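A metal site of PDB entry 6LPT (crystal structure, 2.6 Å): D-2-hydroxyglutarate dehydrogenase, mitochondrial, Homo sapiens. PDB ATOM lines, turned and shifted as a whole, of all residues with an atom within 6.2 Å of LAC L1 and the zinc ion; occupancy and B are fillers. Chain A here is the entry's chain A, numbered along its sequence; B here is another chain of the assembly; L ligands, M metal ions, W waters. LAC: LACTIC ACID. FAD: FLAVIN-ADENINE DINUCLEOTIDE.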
ATOM      1  N   MET A  89     -10.946  12.540  -8.193  1.00  0.00           N
ATOM      2  CA  MET A  89     -11.254  11.263  -7.565  1.00  0.00           C
ATOM      3  C   MET A  89     -10.773  10.066  -8.367  1.00  0.00           C
ATOM      4  O   MET A  89     -10.980   8.926  -7.934  1.00  0.00           O
ATOM      5  CB  MET A  89     -12.756  11.187  -7.287  1.00  0.00           C
ATOM      6  CG  MET A  89     -13.186  12.260  -6.295  1.00  0.00           C
ATOM      7  SD  MET A  89     -13.020  11.798  -4.550  1.00  0.00           S
ATOM      8  CE  MET A  89     -14.731  11.572  -4.096  1.00  0.00           C
ATOM      9  N   GLY A 147     -18.723  20.042  -3.161  1.00  0.00           N
ATOM     10  CA  GLY A 147     -18.169  19.838  -1.831  1.00  0.00           C
ATOM     11  C   GLY A 147     -16.700  20.210  -1.718  1.00  0.00           C
ATOM     12  O   GLY A 147     -16.230  20.569  -0.637  1.00  0.00           O
ATOM     13  N   GLY A 164     -21.910  18.757 -10.093  1.00  0.00           N
ATOM     14  CA  GLY A 164     -22.096  19.326  -8.784  1.00  0.00           C
ATOM     15  C   GLY A 164     -23.542  19.582  -8.405  1.00  0.00           C
ATOM     16  O   GLY A 164     -24.483  19.022  -8.968  1.00  0.00           O
ATOM     17  N   LEU A 165     -23.704  20.474  -7.427  1.00  0.00           N
ATOM     18  CA  LEU A 165     -24.923  20.565  -6.634  1.00  0.00           C
ATOM     19  C   LEU A 165     -25.948  21.528  -7.209  1.00  0.00           C
ATOM     20  O   LEU A 165     -27.095  21.520  -6.749  1.00  0.00           O
ATOM     21  CB  LEU A 165     -24.580  20.976  -5.196  1.00  0.00           C
ATOM     22  CG  LEU A 165     -23.521  20.092  -4.523  1.00  0.00           C
ATOM     23  CD1 LEU A 165     -22.934  20.792  -3.298  1.00  0.00           C
ATOM     24  CD2 LEU A 165     -24.102  18.742  -4.149  1.00  0.00           C
ATOM     25  N   GLU A 265     -31.034  16.485  -4.044  1.00  0.00           N
ATOM     26  CA  GLU A 265     -30.040  15.502  -3.654  1.00  0.00           C
ATOM     27  C   GLU A 265     -30.689  14.471  -2.751  1.00  0.00           C
ATOM     28  O   GLU A 265     -31.677  14.755  -2.081  1.00  0.00           O
ATOM     29  CB  GLU A 265     -28.877  16.172  -2.903  1.00  0.00           C
ATOM     30  CG  GLU A 265     -28.081  17.184  -3.713  1.00  0.00           C
ATOM     31  CD  GLU A 265     -27.263  16.556  -4.801  1.00  0.00           C
ATOM     32  OE1 GLU A 265     -26.625  15.506  -4.544  1.00  0.00           O
ATOM     33  OE2 GLU A 265     -27.232  17.116  -5.913  1.00  0.00           O
ATOM     34  N   ARG A 340     -24.980  16.753   3.441  1.00  0.00           N
ATOM     35  CA  ARG A 340     -24.828  16.165   2.119  1.00  0.00           C
ATOM     36  C   ARG A 340     -23.408  16.328   1.558  1.00  0.00           C
ATOM     37  O   ARG A 340     -22.837  15.358   1.050  1.00  0.00           O
ATOM     38  CB  ARG A 340     -25.860  16.807   1.178  1.00  0.00           C
ATOM     39  CG  ARG A 340     -25.615  16.597  -0.311  1.00  0.00           C
ATOM     40  CD  ARG A 340     -25.600  15.135  -0.697  1.00  0.00           C
ATOM     41  NE  ARG A 340     -25.263  14.998  -2.111  1.00  0.00           N
ATOM     42  CZ  ARG A 340     -24.014  14.960  -2.573  1.00  0.00           C
ATOM     43  NH1 ARG A 340     -22.989  15.007  -1.728  1.00  0.00           N
ATOM     44  NH2 ARG A 340     -23.780  14.851  -3.870  1.00  0.00           N
ATOM     45  N   GLU A 341     -22.866  17.537   1.620  1.00  0.00           N
ATOM     46  CA  GLU A 341     -21.584  17.842   0.986  1.00  0.00           C
ATOM     47  C   GLU A 341     -20.442  16.962   1.494  1.00  0.00           C
ATOM     48  O   GLU A 341     -19.526  16.634   0.737  1.00  0.00           O
ATOM     49  CB  GLU A 341     -21.252  19.310   1.220  1.00  0.00           C
ATOM     50  CG  GLU A 341     -22.075  20.271   0.387  1.00  0.00           C
ATOM     51  CD  GLU A 341     -21.715  21.711   0.666  1.00  0.00           C
ATOM     52  OE1 GLU A 341     -22.026  22.206   1.773  1.00  0.00           O
ATOM     53  OE2 GLU A 341     -21.111  22.349  -0.223  1.00  0.00           O
ATOM     54  N   ILE A 343     -20.505  13.809   2.763  1.00  0.00           N
ATOM     55  CA  ILE A 343     -20.691  12.356   2.818  1.00  0.00           C
ATOM     56  C   ILE A 343     -19.435  11.637   2.334  1.00  0.00           C
ATOM     57  O   ILE A 343     -18.975  10.675   2.955  1.00  0.00           O
ATOM     58  CB  ILE A 343     -21.930  11.957   1.987  1.00  0.00           C
ATOM     59  CG1 ILE A 343     -23.211  12.456   2.663  1.00  0.00           C
ATOM     60  CG2 ILE A 343     -21.978  10.461   1.792  1.00  0.00           C
ATOM     61  CD1 ILE A 343     -24.446  12.341   1.786  1.00  0.00           C
ATOM     62  N   THR A 344     -18.896  12.064   1.191  1.00  0.00           N
ATOM     63  CA  THR A 344     -17.689  11.443   0.629  1.00  0.00           C
ATOM     64  C   THR A 344     -16.523  11.424   1.623  1.00  0.00           C
ATOM     65  O   THR A 344     -15.791  10.431   1.719  1.00  0.00           O
ATOM     66  CB  THR A 344     -17.306  12.146  -0.669  1.00  0.00           C
ATOM     67  OG1 THR A 344     -16.040  11.672  -1.133  1.00  0.00           O
ATOM     68  CG2 THR A 344     -17.254  13.648  -0.462  1.00  0.00           C
ATOM     69  N   LYS A 355     -15.250   3.077  -5.105  1.00  0.00           N
ATOM     70  CA  LYS A 355     -16.011   4.249  -5.513  1.00  0.00           C
ATOM     71  C   LYS A 355     -16.489   4.098  -6.942  1.00  0.00           C
ATOM     72  O   LYS A 355     -15.689   3.871  -7.849  1.00  0.00           O
ATOM     73  CB  LYS A 355     -15.164   5.512  -5.391  1.00  0.00           C
ATOM     74  CG  LYS A 355     -15.940   6.797  -5.636  1.00  0.00           C
ATOM     75  CD  LYS A 355     -15.095   8.006  -5.269  1.00  0.00           C
ATOM     76  CE  LYS A 355     -14.883   8.093  -3.767  1.00  0.00           C
ATOM     77  NZ  LYS A 355     -16.153   8.290  -3.024  1.00  0.00           N
ATOM     78  N   ASP A 357     -19.237   6.013  -9.828  1.00  0.00           N
ATOM     79  CA  ASP A 357     -19.963   7.248 -10.145  1.00  0.00           C
ATOM     80  C   ASP A 357     -20.734   6.956 -11.432  1.00  0.00           C
ATOM     81  O   ASP A 357     -20.170   7.001 -12.524  1.00  0.00           O
ATOM     82  CB  ASP A 357     -18.974   8.403 -10.302  1.00  0.00           C
ATOM     83  CG  ASP A 357     -19.619   9.677 -10.793  1.00  0.00           C
ATOM     84  OD1 ASP A 357     -20.791   9.930 -10.433  1.00  0.00           O
ATOM     85  OD2 ASP A 357     -18.944  10.419 -11.534  1.00  0.00           O
ATOM     86  N   TYR A 386     -25.859   7.617  -2.730  1.00  0.00           N
ATOM     87  CA  TYR A 386     -26.344   8.979  -2.548  1.00  0.00           C
ATOM     88  C   TYR A 386     -26.126   9.747  -3.850  1.00  0.00           C
ATOM     89  O   TYR A 386     -25.678   9.189  -4.839  1.00  0.00           O
ATOM     90  CB  TYR A 386     -25.669   9.651  -1.346  1.00  0.00           C
ATOM     91  CG  TYR A 386     -24.199   9.896  -1.515  1.00  0.00           C
ATOM     92  CD1 TYR A 386     -23.280   8.882  -1.313  1.00  0.00           C
ATOM     93  CD2 TYR A 386     -23.720  11.154  -1.870  1.00  0.00           C
ATOM     94  CE1 TYR A 386     -21.933   9.101  -1.472  1.00  0.00           C
ATOM     95  CE2 TYR A 386     -22.366  11.385  -2.029  1.00  0.00           C
ATOM     96  CZ  TYR A 386     -21.476  10.348  -1.832  1.00  0.00           C
ATOM     97  OH  TYR A 386     -20.125  10.565  -1.982  1.00  0.00           O
ATOM     98  N   GLY A 387     -26.546  11.004  -3.867  1.00  0.00           N
ATOM     99  CA  GLY A 387     -26.085  11.883  -4.931  1.00  0.00           C
ATOM    100  C   GLY A 387     -27.162  12.607  -5.719  1.00  0.00           C
ATOM    101  O   GLY A 387     -28.260  12.859  -5.218  1.00  0.00           O
ATOM    102  N   HIS A 388     -26.831  12.966  -6.967  1.00  0.00           N
ATOM    103  CA  HIS A 388     -27.636  13.905  -7.746  1.00  0.00           C
ATOM    104  C   HIS A 388     -28.753  13.142  -8.450  1.00  0.00           C
ATOM    105  O   HIS A 388     -28.691  12.832  -9.648  1.00  0.00           O
ATOM    106  CB  HIS A 388     -26.765  14.667  -8.720  1.00  0.00           C
ATOM    107  CG  HIS A 388     -25.397  14.969  -8.193  1.00  0.00           C
ATOM    108  ND1 HIS A 388     -25.163  15.989  -7.286  1.00  0.00           N
ATOM    109  CD2 HIS A 388     -24.196  14.400  -8.429  1.00  0.00           C
ATOM    110  CE1 HIS A 388     -23.876  16.030  -7.000  1.00  0.00           C
ATOM    111  NE2 HIS A 388     -23.262  15.075  -7.683  1.00  0.00           N
ATOM    112  N   ASN A 393     -27.712  10.643 -11.291  1.00  0.00           N
ATOM    113  CA  ASN A 393     -26.298  10.412 -11.014  1.00  0.00           C
ATOM    114  C   ASN A 393     -26.187   9.853  -9.605  1.00  0.00           C
ATOM    115  O   ASN A 393     -26.430  10.560  -8.620  1.00  0.00           O
ATOM    116  CB  ASN A 393     -25.484  11.700 -11.154  1.00  0.00           C
ATOM    117  CG  ASN A 393     -23.991  11.500 -10.909  1.00  0.00           C
ATOM    118  OD1 ASN A 393     -23.225  12.466 -10.873  1.00  0.00           O
ATOM    119  ND2 ASN A 393     -23.565  10.246 -10.748  1.00  0.00           N
ATOM    120  N   HIS A 395     -23.828   8.177  -6.686  1.00  0.00           N
ATOM    121  CA  HIS A 395     -22.537   7.892  -6.085  1.00  0.00           C
ATOM    122  C   HIS A 395     -22.747   6.630  -5.275  1.00  0.00           C
ATOM    123  O   HIS A 395     -23.517   6.611  -4.302  1.00  0.00           O
ATOM    124  CB  HIS A 395     -22.057   9.060  -5.219  1.00  0.00           C
ATOM    125  CG  HIS A 395     -21.831  10.327  -5.987  1.00  0.00           C
ATOM    126  ND1 HIS A 395     -21.016  10.386  -7.091  1.00  0.00           N
ATOM    127  CD2 HIS A 395     -22.312  11.574  -5.793  1.00  0.00           C
ATOM    128  CE1 HIS A 395     -21.009  11.623  -7.557  1.00  0.00           C
ATOM    129  NE2 HIS A 395     -21.784  12.361  -6.787  1.00  0.00           N
ATOM    130  N   GLU A 429     -19.460  11.937 -13.572  1.00  0.00           N
ATOM    131  CA  GLU A 429     -18.981  13.248 -13.180  1.00  0.00           C
ATOM    132  C   GLU A 429     -17.468  13.322 -13.078  1.00  0.00           C
ATOM    133  O   GLU A 429     -16.822  14.179 -13.685  1.00  0.00           O
ATOM    134  CB  GLU A 429     -19.537  13.645 -11.820  1.00  0.00           C
ATOM    135  CG  GLU A 429     -20.580  14.710 -11.812  1.00  0.00           C
ATOM    136  CD  GLU A 429     -20.953  15.098 -10.399  1.00  0.00           C
ATOM    137  OE1 GLU A 429     -21.543  16.171 -10.203  1.00  0.00           O
ATOM    138  OE2 GLU A 429     -20.650  14.304  -9.467  1.00  0.00           O
ATOM    139  N   HIS A 430     -16.911  12.393 -12.292  1.00  0.00           N
ATOM    140  CA  HIS A 430     -15.534  12.507 -11.833  1.00  0.00           C
ATOM    141  C   HIS A 430     -14.541  12.345 -12.977  1.00  0.00           C
ATOM    142  O   HIS A 430     -13.401  12.812 -12.863  1.00  0.00           O
ATOM    143  CB  HIS A 430     -15.288  11.467 -10.750  1.00  0.00           C
ATOM    144  CG  HIS A 430     -16.154  11.650  -9.534  1.00  0.00           C
ATOM    145  ND1 HIS A 430     -16.614  10.592  -8.783  1.00  0.00           N
ATOM    146  CD2 HIS A 430     -16.655  12.769  -8.956  1.00  0.00           C
ATOM    147  CE1 HIS A 430     -17.351  11.060  -7.791  1.00  0.00           C
ATOM    148  NE2 HIS A 430     -17.388  12.376  -7.874  1.00  0.00           N
ATOM    149  N   LYS B 198     -25.773  13.118 -17.785  1.00  0.00           N
ATOM    150  CA  LYS B 198     -24.367  13.317 -17.440  1.00  0.00           C
ATOM    151  C   LYS B 198     -23.556  12.099 -17.865  1.00  0.00           C
ATOM    152  O   LYS B 198     -24.000  10.966 -17.685  1.00  0.00           O
ATOM    153  CB  LYS B 198     -24.203  13.576 -15.939  1.00  0.00           C
ATOM    154  CG  LYS B 198     -24.906  14.847 -15.468  1.00  0.00           C
ATOM    155  CD  LYS B 198     -24.933  14.947 -13.962  1.00  0.00           C
ATOM    156  CE  LYS B 198     -23.579  15.240 -13.394  1.00  0.00           C
ATOM    157  NZ  LYS B 198     -23.658  15.473 -11.927  1.00  0.00           N
HETATM  158  C   LAC L   1     -20.588  14.516  -4.530  1.00  0.00           C
HETATM  159  CA  LAC L   1     -19.290  14.022  -5.141  1.00  0.00           C
HETATM  160  CB  LAC L   1     -18.942  12.586  -4.732  1.00  0.00           C
HETATM  161  O   LAC L   1     -21.560  14.880  -5.228  1.00  0.00           O
HETATM  162  OHN LAC L   1     -19.420  14.023  -6.580  1.00  0.00           O
HETATM  163  OXT LAC L   1     -20.638  14.523  -3.290  1.00  0.00           O
HETATM  164  PA  FAD L   2      -7.315  18.311  -9.841  1.00  0.00           P
HETATM  165  O1A FAD L   2      -6.075  18.981  -9.375  1.00  0.00           O
HETATM  166  O2A FAD L   2      -7.879  17.212  -8.916  1.00  0.00           O
HETATM  167  O5B FAD L   2      -7.181  17.737 -11.269  1.00  0.00           O
HETATM  168  C5B FAD L   2      -8.220  16.909 -11.837  1.00  0.00           C
HETATM  169  C4B FAD L   2      -7.862  16.470 -13.237  1.00  0.00           C
HETATM  170  O4B FAD L   2      -7.889  17.606 -14.124  1.00  0.00           O
HETATM  171  C3B FAD L   2      -6.487  15.839 -13.425  1.00  0.00           C
HETATM  172  O3B FAD L   2      -6.510  14.922 -14.503  1.00  0.00           O
HETATM  173  C2B FAD L   2      -5.611  17.059 -13.748  1.00  0.00           C
HETATM  174  O2B FAD L   2      -4.472  16.687 -14.512  1.00  0.00           O
HETATM  175  C1B FAD L   2      -6.571  17.917 -14.570  1.00  0.00           C
HETATM  176  N9A FAD L   2      -6.379  19.356 -14.417  1.00  0.00           N
HETATM  177  C8A FAD L   2      -6.416  20.089 -13.256  1.00  0.00           C
HETATM  178  N7A FAD L   2      -6.216  21.378 -13.433  1.00  0.00           N
HETATM  179  C5A FAD L   2      -6.029  21.501 -14.794  1.00  0.00           C
HETATM  180  C6A FAD L   2      -5.777  22.612 -15.627  1.00  0.00           C
HETATM  181  N6A FAD L   2      -5.658  23.866 -15.192  1.00  0.00           N
HETATM  182  N1A FAD L   2      -5.637  22.379 -16.958  1.00  0.00           N
HETATM  183  C2A FAD L   2      -5.756  21.135 -17.413  1.00  0.00           C
HETATM  184  N3A FAD L   2      -6.000  20.010 -16.723  1.00  0.00           N
HETATM  185  C4A FAD L   2      -6.123  20.267 -15.416  1.00  0.00           C
HETATM  186  N1  FAD L   2     -16.861  16.349  -8.782  1.00  0.00           N
HETATM  187  C2  FAD L   2     -18.042  16.618  -9.402  1.00  0.00           C
HETATM  188  O2  FAD L   2     -18.163  16.559 -10.629  1.00  0.00           O
HETATM  189  N3  FAD L   2     -19.160  16.941  -8.645  1.00  0.00           N
HETATM  190  C4  FAD L   2     -19.202  17.044  -7.274  1.00  0.00           C
HETATM  191  O4  FAD L   2     -20.251  17.338  -6.712  1.00  0.00           O
HETATM  192  C4X FAD L   2     -17.927  16.778  -6.620  1.00  0.00           C
HETATM  193  N5  FAD L   2     -17.885  16.857  -5.329  1.00  0.00           N
HETATM  194  C5X FAD L   2     -16.682  16.608  -4.701  1.00  0.00           C
HETATM  195  C6  FAD L   2     -16.629  16.687  -3.308  1.00  0.00           C
HETATM  196  C7  FAD L   2     -15.436  16.445  -2.623  1.00  0.00           C
HETATM  197  C7M FAD L   2     -15.418  16.547  -1.116  1.00  0.00           C
HETATM  198  C8  FAD L   2     -14.278  16.110  -3.346  1.00  0.00           C
HETATM  199  C8M FAD L   2     -12.986  15.840  -2.630  1.00  0.00           C
HETATM  200  C9  FAD L   2     -14.327  16.028  -4.731  1.00  0.00           C
HETATM  201  C9A FAD L   2     -15.516  16.276  -5.404  1.00  0.00           C
HETATM  202  N10 FAD L   2     -15.592  16.205  -6.818  1.00  0.00           N
HETATM  203  C10 FAD L   2     -16.806  16.437  -7.459  1.00  0.00           C
HETATM  204  C1' FAD L   2     -14.399  15.838  -7.610  1.00  0.00           C
HETATM  205  C2' FAD L   2     -14.087  16.814  -8.748  1.00  0.00           C
HETATM  206  O2' FAD L   2     -13.585  16.107  -9.887  1.00  0.00           O
HETATM  207  C3' FAD L   2     -13.075  17.870  -8.304  1.00  0.00           C
HETATM  208  O3' FAD L   2     -13.286  18.205  -6.941  1.00  0.00           O
HETATM  209  C4' FAD L   2     -13.223  19.126  -9.161  1.00  0.00           C
HETATM  210  O4' FAD L   2     -13.584  18.744 -10.493  1.00  0.00           O
HETATM  211  C5' FAD L   2     -12.028  20.056  -9.195  1.00  0.00           C
HETATM  212  O5' FAD L   2     -10.815  19.288  -9.299  1.00  0.00           O
HETATM  213  P   FAD L   2      -9.415  19.941  -8.940  1.00  0.00           P
HETATM  214  O1P FAD L   2      -9.487  21.456  -9.107  1.00  0.00           O
HETATM  215  O2P FAD L   2      -8.946  19.476  -7.606  1.00  0.00           O
HETATM  216  O3P FAD L   2      -8.454  19.385 -10.067  1.00  0.00           O
HETATM  217 ZN    ZN M   1     -21.296  14.531  -7.194  1.00  0.00          ZN
HETATM  218  O   HOH W   1     -18.556   9.236  -4.152  1.00  0.00           O
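OD1 of Asn 393 lies close to OE2 of Glu 429.
The side-chain carboxylate of Asp 357 sits at hydrogen-bond distance from the backbone NH of Glu 429, at 2.6 Å.
The backbone carbonyl oxygen (O) of Tyr 386 is in hydrogen-bond range of the backbone NH (N) of His 395, 2.8 Å away.
The side-chain carboxylate (OE2) of Glu 265 is in hydrogen-bond range of a ring nitrogen (ND1) of His 388 (2.7 Å).
OE1 of Glu 429 is in hydrogen-bond range of N of Gly 164, 2.6 Å away.
The backbone NH of His 430 lies within hydrogen-bond range of the side-chain carboxylate of Asp 357 (2.9 Å).
The backbone NH (N) of Asn 393 sits at hydrogen-bond distance from the backbone carbonyl oxygen (O) of His 388 (2.9 Å).
OE1 of Glu 429 is in salt-bridge range of NZ of Lys 198 of chain B, 2.8 Å away.
Of the 19 residues printed, 3 come within 4 Å of the zinc ion.
The nearest printed residue that does not touch the zinc ion is Arg 340 (4.2 Å).
Tyr 386 touches LAC L1.
Hydrophobic or aromatic side chains that line LAC L1: Tyr 386, His 388, His 395 and His 430.
Within 4 Å of LAC L1: Arg 340, Tyr 386, His 388, His 395, Glu 429 and His 430.
The nearest printed residue that does not touch LAC L1 is Met 89 (4.4 Å).
The zinc ion is bound by O of LAC L1 (2.0 Å), OHN of LAC L1 (2.0 Å), NE2 of His 388 (2.1 Å), NE2 of His 395 (2.3 Å) and OE2 of Glu 429 (2.4 Å).
The zinc ion has five donor atoms within binding distance.
Water W1 bridges NZ of Lys 355 (2.8 Å) and OH of Tyr 386 (3.0 Å).
An oxygen (O4) of FAD L2 sits close to an oxygen (OHN) of LAC L1, at 3.4 Å.
A ring nitrogen (NE2) of His 430 sits close to an oxygen (OHN) of LAC L1 (2.9 Å).
An oxygen (OXT) of LAC L1 lies within salt-bridge range of the guanidinium group (NH1) of Arg 340, 2.9 Å away.
The side-chain carboxylate (OE1) of Glu 429 lies within hydrogen-bond range of a nitrogen (N3) of FAD L2 (2.9 Å).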
